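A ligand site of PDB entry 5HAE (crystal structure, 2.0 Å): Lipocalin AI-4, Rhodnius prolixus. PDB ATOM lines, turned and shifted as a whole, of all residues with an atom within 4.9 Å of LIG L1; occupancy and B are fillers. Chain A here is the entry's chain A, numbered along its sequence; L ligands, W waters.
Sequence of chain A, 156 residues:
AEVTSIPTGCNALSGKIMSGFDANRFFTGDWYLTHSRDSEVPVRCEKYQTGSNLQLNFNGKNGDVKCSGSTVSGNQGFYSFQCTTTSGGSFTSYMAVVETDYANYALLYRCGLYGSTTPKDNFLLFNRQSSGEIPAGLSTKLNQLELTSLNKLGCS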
ATOM      1  N   PHE A  26      17.854  -8.693   2.479  1.00  0.00           N
ATOM      2  CA  PHE A  26      17.155  -7.864   1.512  1.00  0.00           C
ATOM      3  C   PHE A  26      17.895  -6.568   1.142  1.00  0.00           C
ATOM      4  O   PHE A  26      17.973  -6.222  -0.042  1.00  0.00           O
ATOM      5  CB  PHE A  26      15.749  -7.490   2.003  1.00  0.00           C
ATOM      6  CG  PHE A  26      15.053  -6.534   1.064  1.00  0.00           C
ATOM      7  CD1 PHE A  26      14.522  -6.987  -0.128  1.00  0.00           C
ATOM      8  CD2 PHE A  26      14.957  -5.183   1.374  1.00  0.00           C
ATOM      9  CE1 PHE A  26      13.896  -6.126  -1.011  1.00  0.00           C
ATOM     10  CE2 PHE A  26      14.334  -4.293   0.496  1.00  0.00           C
ATOM     11  CZ  PHE A  26      13.805  -4.762  -0.702  1.00  0.00           C
ATOM     12  N   TRP A  31      18.700  -3.493  -6.685  1.00  0.00           N
ATOM     13  CA  TRP A  31      17.335  -3.911  -7.011  1.00  0.00           C
ATOM     14  C   TRP A  31      16.772  -3.048  -8.144  1.00  0.00           C
ATOM     15  O   TRP A  31      16.693  -1.822  -8.006  1.00  0.00           O
ATOM     16  CB  TRP A  31      16.409  -3.808  -5.787  1.00  0.00           C
ATOM     17  CG  TRP A  31      16.551  -4.904  -4.737  1.00  0.00           C
ATOM     18  CD1 TRP A  31      17.113  -4.781  -3.497  1.00  0.00           C
ATOM     19  CD2 TRP A  31      16.053  -6.254  -4.829  1.00  0.00           C
ATOM     20  NE1 TRP A  31      17.029  -5.979  -2.819  1.00  0.00           N
ATOM     21  CE2 TRP A  31      16.376  -6.899  -3.611  1.00  0.00           C
ATOM     22  CE3 TRP A  31      15.367  -6.975  -5.814  1.00  0.00           C
ATOM     23  CZ2 TRP A  31      16.040  -8.241  -3.357  1.00  0.00           C
ATOM     24  CZ3 TRP A  31      15.051  -8.309  -5.562  1.00  0.00           C
ATOM     25  CH2 TRP A  31      15.383  -8.921  -4.359  1.00  0.00           C
ATOM     26  N   GLU A  40       3.889   5.780 -14.148  1.00  0.00           N
ATOM     27  CA  GLU A  40       3.858   7.055 -14.834  1.00  0.00           C
ATOM     28  C   GLU A  40       4.258   6.877 -16.281  1.00  0.00           C
ATOM     29  O   GLU A  40       4.680   5.786 -16.668  1.00  0.00           O
ATOM     30  CB  GLU A  40       4.814   8.066 -14.183  1.00  0.00           C
ATOM     31  CG  GLU A  40       5.059   7.875 -12.703  1.00  0.00           C
ATOM     32  CD  GLU A  40       6.298   8.624 -12.230  1.00  0.00           C
ATOM     33  OE1 GLU A  40       7.389   8.422 -12.812  1.00  0.00           O
ATOM     34  OE2 GLU A  40       6.176   9.429 -11.274  1.00  0.00           O
ATOM     35  N   TYR A  48      17.845   0.659  -7.705  1.00  0.00           N
ATOM     36  CA  TYR A  48      18.020   0.977  -6.296  1.00  0.00           C
ATOM     37  C   TYR A  48      19.299   0.321  -5.781  1.00  0.00           C
ATOM     38  O   TYR A  48      19.412  -0.919  -5.727  1.00  0.00           O
ATOM     39  CB  TYR A  48      16.786   0.541  -5.471  1.00  0.00           C
ATOM     40  CG  TYR A  48      15.580   1.412  -5.749  1.00  0.00           C
ATOM     41  CD1 TYR A  48      14.955   1.403  -6.997  1.00  0.00           C
ATOM     42  CD2 TYR A  48      15.066   2.252  -4.775  1.00  0.00           C
ATOM     43  CE1 TYR A  48      13.848   2.223  -7.272  1.00  0.00           C
ATOM     44  CE2 TYR A  48      13.964   3.066  -5.022  1.00  0.00           C
ATOM     45  CZ  TYR A  48      13.356   3.052  -6.270  1.00  0.00           C
ATOM     46  OH  TYR A  48      12.274   3.869  -6.506  1.00  0.00           O
ATOM     47  N   THR A  50      21.859  -0.347  -2.695  1.00  0.00           N
ATOM     48  CA  THR A  50      21.807  -0.379  -1.233  1.00  0.00           C
ATOM     49  C   THR A  50      23.193  -0.323  -0.594  1.00  0.00           C
ATOM     50  O   THR A  50      24.185  -0.649  -1.227  1.00  0.00           O
ATOM     51  CB  THR A  50      21.111  -1.650  -0.700  1.00  0.00           C
ATOM     52  OG1 THR A  50      21.910  -2.800  -1.024  1.00  0.00           O
ATOM     53  CG2 THR A  50      19.739  -1.810  -1.290  1.00  0.00           C
ATOM     54  N   LEU A  56      20.226   4.100   0.791  1.00  0.00           N
ATOM     55  CA  LEU A  56      20.084   3.707  -0.602  1.00  0.00           C
ATOM     56  C   LEU A  56      20.186   4.881  -1.563  1.00  0.00           C
ATOM     57  O   LEU A  56      19.988   6.039  -1.178  1.00  0.00           O
ATOM     58  CB  LEU A  56      18.774   2.929  -0.821  1.00  0.00           C
ATOM     59  CG  LEU A  56      17.393   3.446  -0.450  1.00  0.00           C
ATOM     60  CD1 LEU A  56      16.854   4.343  -1.542  1.00  0.00           C
ATOM     61  CD2 LEU A  56      16.479   2.275  -0.242  1.00  0.00           C
ATOM     62  N   PHE A  58      19.061   5.863  -5.689  1.00  0.00           N
ATOM     63  CA  PHE A  58      18.506   5.445  -6.976  1.00  0.00           C
ATOM     64  C   PHE A  58      18.448   6.606  -7.934  1.00  0.00           C
ATOM     65  O   PHE A  58      18.511   7.765  -7.525  1.00  0.00           O
ATOM     66  CB  PHE A  58      17.124   4.797  -6.807  1.00  0.00           C
ATOM     67  CG  PHE A  58      16.029   5.746  -6.392  1.00  0.00           C
ATOM     68  CD1 PHE A  58      15.837   6.054  -5.046  1.00  0.00           C
ATOM     69  CD2 PHE A  58      15.161   6.281  -7.322  1.00  0.00           C
ATOM     70  CE1 PHE A  58      14.805   6.893  -4.659  1.00  0.00           C
ATOM     71  CE2 PHE A  58      14.137   7.131  -6.944  1.00  0.00           C
ATOM     72  CZ  PHE A  58      13.962   7.434  -5.598  1.00  0.00           C
ATOM     73  N   LYS A  61      13.423  10.529 -10.922  1.00  0.00           N
ATOM     74  CA  LYS A  61      12.796  11.234 -12.040  1.00  0.00           C
ATOM     75  C   LYS A  61      13.671  12.339 -12.601  1.00  0.00           C
ATOM     76  O   LYS A  61      13.777  12.498 -13.813  1.00  0.00           O
ATOM     77  CB  LYS A  61      11.445  11.823 -11.610  1.00  0.00           C
ATOM     78  CG  LYS A  61      10.248  10.955 -11.953  1.00  0.00           C
ATOM     79  CD  LYS A  61       9.015  11.365 -11.164  1.00  0.00           C
ATOM     80  CE  LYS A  61       9.175  11.067  -9.671  1.00  0.00           C
ATOM     81  NZ  LYS A  61       7.900  11.295  -8.906  1.00  0.00           N
ATOM     82  N   CYS A  67      18.532   8.163   0.081  1.00  0.00           N
ATOM     83  CA  CYS A  67      17.622   7.925   1.190  1.00  0.00           C
ATOM     84  C   CYS A  67      18.308   7.252   2.359  1.00  0.00           C
ATOM     85  O   CYS A  67      19.217   6.437   2.167  1.00  0.00           O
ATOM     86  CB  CYS A  67      16.436   7.067   0.743  1.00  0.00           C
ATOM     87  SG  CYS A  67      15.575   7.655  -0.699  1.00  0.00           S
ATOM     88  N   PHE A  81      11.806   6.043   4.951  1.00  0.00           N
ATOM     89  CA  PHE A  81      13.000   6.572   4.282  1.00  0.00           C
ATOM     90  C   PHE A  81      12.930   8.089   4.156  1.00  0.00           C
ATOM     91  O   PHE A  81      11.929   8.640   3.705  1.00  0.00           O
ATOM     92  CB  PHE A  81      13.182   5.903   2.919  1.00  0.00           C
ATOM     93  CG  PHE A  81      13.749   4.521   3.020  1.00  0.00           C
ATOM     94  CD1 PHE A  81      12.916   3.431   3.172  1.00  0.00           C
ATOM     95  CD2 PHE A  81      15.132   4.327   3.030  1.00  0.00           C
ATOM     96  CE1 PHE A  81      13.441   2.145   3.306  1.00  0.00           C
ATOM     97  CE2 PHE A  81      15.668   3.060   3.166  1.00  0.00           C
ATOM     98  CZ  PHE A  81      14.820   1.960   3.311  1.00  0.00           C
ATOM     99  N   CYS A  83      14.431  10.929   2.127  1.00  0.00           N
ATOM    100  CA  CYS A  83      15.151  11.074   0.857  1.00  0.00           C
ATOM    101  C   CYS A  83      15.396  12.512   0.474  1.00  0.00           C
ATOM    102  O   CYS A  83      14.579  13.404   0.749  1.00  0.00           O
ATOM    103  CB  CYS A  83      14.390  10.389  -0.290  1.00  0.00           C
ATOM    104  SG  CYS A  83      13.960   8.663  -0.002  1.00  0.00           S
ATOM    105  N   PHE A  91      11.902  14.511   0.949  1.00  0.00           N
ATOM    106  CA  PHE A  91      10.634  13.849   1.238  1.00  0.00           C
ATOM    107  C   PHE A  91      10.801  12.583   2.050  1.00  0.00           C
ATOM    108  O   PHE A  91      11.904  12.020   2.146  1.00  0.00           O
ATOM    109  CB  PHE A  91       9.869  13.514  -0.054  1.00  0.00           C
ATOM    110  CG  PHE A  91      10.553  12.479  -0.922  1.00  0.00           C
ATOM    111  CD1 PHE A  91      11.481  12.875  -1.871  1.00  0.00           C
ATOM    112  CD2 PHE A  91      10.232  11.127  -0.811  1.00  0.00           C
ATOM    113  CE1 PHE A  91      12.088  11.941  -2.692  1.00  0.00           C
ATOM    114  CE2 PHE A  91      10.851  10.190  -1.624  1.00  0.00           C
ATOM    115  CZ  PHE A  91      11.782  10.599  -2.575  1.00  0.00           C
ATOM    116  N   SER A  93       9.184   8.602   2.674  1.00  0.00           N
ATOM    117  CA  SER A  93       8.432   7.530   2.007  1.00  0.00           C
ATOM    118  C   SER A  93       8.449   6.283   2.867  1.00  0.00           C
ATOM    119  O   SER A  93       9.417   6.033   3.601  1.00  0.00           O
ATOM    120  CB  SER A  93       9.014   7.245   0.613  1.00  0.00           C
ATOM    121  OG  SER A  93       8.170   6.357  -0.111  1.00  0.00           O
ATOM    122  N   MET A  95       7.689   2.000   3.333  1.00  0.00           N
ATOM    123  CA  MET A  95       7.709   0.788   2.534  1.00  0.00           C
ATOM    124  C   MET A  95       7.694  -0.465   3.388  1.00  0.00           C
ATOM    125  O   MET A  95       8.177  -0.455   4.514  1.00  0.00           O
ATOM    126  CB  MET A  95       8.944   0.789   1.636  1.00  0.00           C
ATOM    127  CG  MET A  95      10.186   0.513   2.469  1.00  0.00           C
ATOM    128  SD  MET A  95      11.304  -0.564   1.623  1.00  0.00           S
ATOM    129  CE  MET A  95      10.581  -2.071   2.155  1.00  0.00           C
ATOM    130  N   LEU A 108       7.098  -5.246  -3.063  1.00  0.00           N
ATOM    131  CA  LEU A 108       7.055  -4.247  -2.004  1.00  0.00           C
ATOM    132  C   LEU A 108       5.771  -3.432  -2.026  1.00  0.00           C
ATOM    133  O   LEU A 108       5.103  -3.327  -3.054  1.00  0.00           O
ATOM    134  CB  LEU A 108       8.248  -3.288  -2.118  1.00  0.00           C
ATOM    135  CG  LEU A 108       9.560  -3.689  -1.461  1.00  0.00           C
ATOM    136  CD1 LEU A 108      10.157  -4.907  -2.116  1.00  0.00           C
ATOM    137  CD2 LEU A 108      10.565  -2.543  -1.500  1.00  0.00           C
ATOM    138  N   ARG A 110       4.603   0.510  -1.057  1.00  0.00           N
ATOM    139  CA  ARG A 110       5.172   1.829  -0.770  1.00  0.00           C
ATOM    140  C   ARG A 110       4.048   2.836  -0.603  1.00  0.00           C
ATOM    141  O   ARG A 110       3.043   2.774  -1.311  1.00  0.00           O
ATOM    142  CB  ARG A 110       6.128   2.266  -1.893  1.00  0.00           C
ATOM    143  CG  ARG A 110       6.789   3.614  -1.630  1.00  0.00           C
ATOM    144  CD  ARG A 110       7.998   3.836  -2.531  1.00  0.00           C
ATOM    145  NE  ARG A 110       7.605   4.004  -3.926  1.00  0.00           N
ATOM    146  CZ  ARG A 110       8.486   4.002  -4.929  1.00  0.00           C
ATOM    147  NH1 ARG A 110       9.781   3.848  -4.683  1.00  0.00           N
ATOM    148  NH2 ARG A 110       8.049   4.144  -6.176  1.00  0.00           N
ATOM    149  N   TYR A 114       3.566  12.814   0.784  1.00  0.00           N
ATOM    150  CA  TYR A 114       4.297  13.740  -0.091  1.00  0.00           C
ATOM    151  C   TYR A 114       3.655  15.126  -0.143  1.00  0.00           C
ATOM    152  O   TYR A 114       3.400  15.677  -1.211  1.00  0.00           O
ATOM    153  CB  TYR A 114       4.415  13.130  -1.496  1.00  0.00           C
ATOM    154  CG  TYR A 114       4.834  11.681  -1.454  1.00  0.00           C
ATOM    155  CD1 TYR A 114       6.119  11.308  -1.059  1.00  0.00           C
ATOM    156  CD2 TYR A 114       3.938  10.669  -1.780  1.00  0.00           C
ATOM    157  CE1 TYR A 114       6.499   9.991  -0.991  1.00  0.00           C
ATOM    158  CE2 TYR A 114       4.318   9.330  -1.707  1.00  0.00           C
ATOM    159  CZ  TYR A 114       5.591   8.997  -1.318  1.00  0.00           C
ATOM    160  OH  TYR A 114       5.960   7.683  -1.259  1.00  0.00           O
ATOM    161  N   LYS A 120      -0.407   8.568  -1.459  1.00  0.00           N
ATOM    162  CA  LYS A 120      -0.170   7.892  -2.727  1.00  0.00           C
ATOM    163  C   LYS A 120       0.555   6.596  -2.469  1.00  0.00           C
ATOM    164  O   LYS A 120       1.594   6.598  -1.833  1.00  0.00           O
ATOM    165  CB  LYS A 120       0.626   8.766  -3.705  1.00  0.00           C
ATOM    166  CG  LYS A 120      -0.132   9.999  -4.025  1.00  0.00           C
ATOM    167  CD  LYS A 120      -1.401   9.549  -4.716  1.00  0.00           C
ATOM    168  CE  LYS A 120      -2.285  10.692  -5.112  1.00  0.00           C
ATOM    169  NZ  LYS A 120      -2.884  11.378  -3.920  1.00  0.00           N
ATOM    170  N   ASP A 121       0.004   5.479  -2.920  1.00  0.00           N
ATOM    171  CA  ASP A 121       0.693   4.229  -2.685  1.00  0.00           C
ATOM    172  C   ASP A 121       0.814   3.403  -3.946  1.00  0.00           C
ATOM    173  O   ASP A 121       0.354   3.806  -5.015  1.00  0.00           O
ATOM    174  CB  ASP A 121       0.025   3.437  -1.532  1.00  0.00           C
ATOM    175  CG  ASP A 121      -1.393   2.962  -1.850  1.00  0.00           C
ATOM    176  OD1 ASP A 121      -1.842   3.066  -2.999  1.00  0.00           O
ATOM    177  OD2 ASP A 121      -2.046   2.456  -0.910  1.00  0.00           O
ATOM    178  N   ASN A 122       1.475   2.254  -3.815  1.00  0.00           N
ATOM    179  CA  ASN A 122       1.777   1.409  -4.951  1.00  0.00           C
ATOM    180  C   ASN A 122       2.215   0.032  -4.485  1.00  0.00           C
ATOM    181  O   ASN A 122       2.638  -0.145  -3.333  1.00  0.00           O
ATOM    182  CB  ASN A 122       2.871   2.052  -5.819  1.00  0.00           C
ATOM    183  CG  ASN A 122       2.627   1.858  -7.303  1.00  0.00           C
ATOM    184  OD1 ASN A 122       1.838   1.014  -7.706  1.00  0.00           O
ATOM    185  ND2 ASN A 122       3.315   2.652  -8.132  1.00  0.00           N
ATOM    186  N   LEU A 124       5.064  -2.591  -5.803  1.00  0.00           N
ATOM    187  CA  LEU A 124       6.264  -2.535  -6.616  1.00  0.00           C
ATOM    188  C   LEU A 124       6.916  -3.905  -6.742  1.00  0.00           C
ATOM    189  O   LEU A 124       7.091  -4.594  -5.745  1.00  0.00           O
ATOM    190  CB  LEU A 124       7.266  -1.570  -5.998  1.00  0.00           C
ATOM    191  CG  LEU A 124       6.791  -0.168  -5.606  1.00  0.00           C
ATOM    192  CD1 LEU A 124       7.877   0.546  -4.797  1.00  0.00           C
ATOM    193  CD2 LEU A 124       6.399   0.614  -6.830  1.00  0.00           C
ATOM    194  N   PHE A 126      10.398  -5.621  -7.635  1.00  0.00           N
ATOM    195  CA  PHE A 126      11.826  -5.426  -7.834  1.00  0.00           C
ATOM    196  C   PHE A 126      12.449  -6.729  -8.283  1.00  0.00           C
ATOM    197  O   PHE A 126      12.014  -7.808  -7.895  1.00  0.00           O
ATOM    198  CB  PHE A 126      12.511  -4.935  -6.548  1.00  0.00           C
ATOM    199  CG  PHE A 126      12.117  -3.526  -6.146  1.00  0.00           C
ATOM    200  CD1 PHE A 126      10.998  -3.303  -5.346  1.00  0.00           C
ATOM    201  CD2 PHE A 126      12.866  -2.437  -6.563  1.00  0.00           C
ATOM    202  CE1 PHE A 126      10.646  -2.013  -4.970  1.00  0.00           C
ATOM    203  CE2 PHE A 126      12.511  -1.138  -6.191  1.00  0.00           C
ATOM    204  CZ  PHE A 126      11.405  -0.934  -5.391  1.00  0.00           C
HETATM  205  O1  LIG L   1       5.167   4.494  -6.723  1.00  0.00           O
HETATM  206  C1  LIG L   1       4.586   4.959  -5.700  1.00  0.00           C
HETATM  207  O2  LIG L   1       4.967   4.623  -4.554  1.00  0.00           O
HETATM  208  C2  LIG L   1       3.420   5.910  -5.867  1.00  0.00           C
HETATM  209  C3  LIG L   1       3.925   7.259  -6.321  1.00  0.00           C
HETATM  210  C4  LIG L   1       5.327   7.409  -5.817  1.00  0.00           C
HETATM  211  C5  LIG L   1       5.732   8.831  -5.716  1.00  0.00           C
HETATM  212  O3  LIG L   1       6.446   9.226  -6.866  1.00  0.00           O
HETATM  213  C6  LIG L   1       6.594   8.868  -4.465  1.00  0.00           C
HETATM  214  C7  LIG L   1       8.034   8.499  -4.732  1.00  0.00           C
HETATM  215  C8  LIG L   1       8.787   8.128  -3.677  1.00  0.00           C
HETATM  216  C9  LIG L   1      10.012   7.281  -3.862  1.00  0.00           C
HETATM  217  C10 LIG L   1      10.601   6.700  -2.801  1.00  0.00           C
HETATM  218  C11 LIG L   1      11.920   5.993  -3.015  1.00  0.00           C
HETATM  219  C12 LIG L   1      12.530   5.310  -2.021  1.00  0.00           C
HETATM  220  C13 LIG L   1      11.956   5.194  -0.622  1.00  0.00           C
HETATM  221  C14 LIG L   1      10.872   4.124  -0.580  1.00  0.00           C
HETATM  222  C15 LIG L   1      11.104   2.798  -0.670  1.00  0.00           C
HETATM  223  C16 LIG L   1      12.497   2.209  -0.824  1.00  0.00           C
HETATM  224  C17 LIG L   1      12.468   0.982  -1.697  1.00  0.00           C
HETATM  225  C18 LIG L   1      13.787   0.265  -1.550  1.00  0.00           C
HETATM  226  C19 LIG L   1      13.872  -0.933  -2.469  1.00  0.00           C
HETATM  227  C20 LIG L   1      15.241  -1.556  -2.352  1.00  0.00           C
HETATM  228  N1  LG2 L   2       3.748  17.349  -4.924  1.00  0.00           N
HETATM  229  C1  LG2 L   2       4.588  17.857  -3.920  1.00  0.00           C
HETATM  230  C2  LG2 L   2       5.419  18.996  -4.493  1.00  0.00           C
HETATM  231  O1  LG2 L   2       5.445  19.175  -5.735  1.00  0.00           O
HETATM  232  O2  LG2 L   2       6.073  19.765  -3.731  1.00  0.00           O
HETATM  233  C3  LG2 L   2       5.522  16.779  -3.380  1.00  0.00           C
HETATM  234  C4  LG2 L   2       6.299  16.099  -4.514  1.00  0.00           C
HETATM  235  C5  LG2 L   2       7.310  15.152  -3.915  1.00  0.00           C
HETATM  236  O3  LG2 L   2       7.577  15.141  -2.733  1.00  0.00           O
HETATM  237  N2  LG2 L   2       7.991  14.208  -4.772  1.00  0.00           N
HETATM  238  C6  LG2 L   2       8.971  13.304  -4.203  1.00  0.00           C
HETATM  239  C7  LG2 L   2      10.161  13.327  -5.158  1.00  0.00           C
HETATM  240  O4  LG2 L   2      10.765  14.365  -5.385  1.00  0.00           O
HETATM  241  C8  LG2 L   2       8.389  11.946  -4.080  1.00  0.00           C
HETATM  242  S1  LG2 L   2       7.283  11.694  -5.469  1.00  0.00           S
HETATM  243  N3  LG2 L   2      10.565  12.127  -5.814  1.00  0.00           N
HETATM  244  C9  LG2 L   2      11.679  12.170  -6.712  1.00  0.00           C
HETATM  245  C10 LG2 L   2      11.800  10.779  -7.295  1.00  0.00           C
HETATM  246  O5  LG2 L   2      12.691  10.528  -8.153  1.00  0.00           O
HETATM  247  O6  LG2 L   2      11.024   9.888  -6.900  1.00  0.00           O
HETATM  248  O   HOH W   1       4.324   6.026  -2.228  1.00  0.00           O
HETATM  249  O   HOH W   2       5.159   5.166  -9.279  1.00  0.00           O
HETATM  250  O   HOH W   3       4.546   9.456  -9.184  1.00  0.00           O
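O2 of LIG L1 is in salt-bridge range of NE of Arg 110, at 2.8 Å. An oxygen (O1) of LIG L1 sits at hydrogen-bond distance from the side-chain amide nitrogen (ND2) of Asn 122. The side-chain amino group (NZ) of Lys 61 lies within hydrogen-bond range of an oxygen (O3) of LIG L1, at 3.2 Å. The backbone NH (N) of Lys 61 sits at hydrogen-bond distance from an oxygen (O5) of LG2 L2 (2.9 Å). The side-chain amino group of Lys 61 is in salt-bridge range of an oxygen (O6) of LG2 L2 (3.97 Å).
O3 of LIG L1 lies close to S1 of LG2 L2.
The backbone carbonyl oxygen (O) of Arg 110 is in hydrogen-bond range of the backbone NH (N) of Asn 122, at 3.0 Å. The guanidinium group (NH1) of Arg 110 is in hydrogen-bond range of the side-chain hydroxyl (OH) of Tyr 48 (3.1 Å). The side-chain hydroxyl of Tyr 114 is in hydrogen-bond range of the side-chain hydroxyl of Ser 93 (2.8 Å). The backbone NH (N) of Phe 81 is in hydrogen-bond range of the backbone carbonyl oxygen (O) of Ser 93 (2.7 Å). O of Phe 91 sits at hydrogen-bond distance from N of Cys 83, 2.8 Å away. O of Leu 56 sits at hydrogen-bond distance from N of Cys 67. The backbone carbonyl oxygen of Phe 26 is in hydrogen-bond range of the indole nitrogen of Trp 31 (2.9 Å). The side-chain sulfur (SG) of Cys 67 forms a disulfide with the side-chain sulfur (SG) of Cys 83 (2.0 Å).
Phe 26 touches LIG L1 (CZ to C20, 3.9 Å). Trp 31 touches LIG L1. CD2 of Tyr 48 touches C18 of LIG L1, at 3.998 Å. CD2 of Leu 56 touches C18 of LIG L1 (3.6 Å). Phe 58 touches LIG L1 (CE1 to C11, 3.4 Å). CB of Phe 81 touches C13 of LIG L1, 3.8 Å away. CE2 of Phe 91 touches C8 of LIG L1 (3.6 Å). Ser 93 touches LIG L1 (OG to C14, 3.5 Å). Met 95 touches LIG L1 (CB to C15, 3.7 Å). Leu 108 touches LIG L1. CZ of Tyr 114 touches C6 of LIG L1, 3.3 Å away. Asp 121 touches LIG L1 (O to C2, 3.8 Å). Phe 126 touches LIG L1 (CZ to C19, 3.8 Å). Hydrophobic or aromatic side chains within 4 Å of LIG L1: Phe 26, Trp 31, Tyr 48, Leu 56, Phe 58, Phe 81, Phe 91, Met 95, Leu 108, Tyr 114 and Phe 126. Within 4 Å of LIG L1: Phe 26, Trp 31, Tyr 48, Leu 56, Phe 58, Lys 61, Phe 81, Phe 91, Ser 93, Met 95, Leu 108, Arg 110, Tyr 114, Asp 121, Asn 122 and Phe 126. The nearest printed residue that does not touch LIG L1 is Cys 83 (4.1 Å).
Water W2 lies within hydrogen-bond range of an oxygen (O1) of LIG L1 (2.6 Å) and the side-chain amide nitrogen (ND2) of Asn 122 (3.3 Å). Water W1 lies within hydrogen-bond range of OH of Tyr 114 (2.5 Å), O2 of LIG L1 (2.8 Å) and O of Lys 120 (2.8 Å). Water W3 lies within hydrogen-bond range of the side-chain carboxylate of Glu 40 and an oxygen (O3) of LIG L1.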
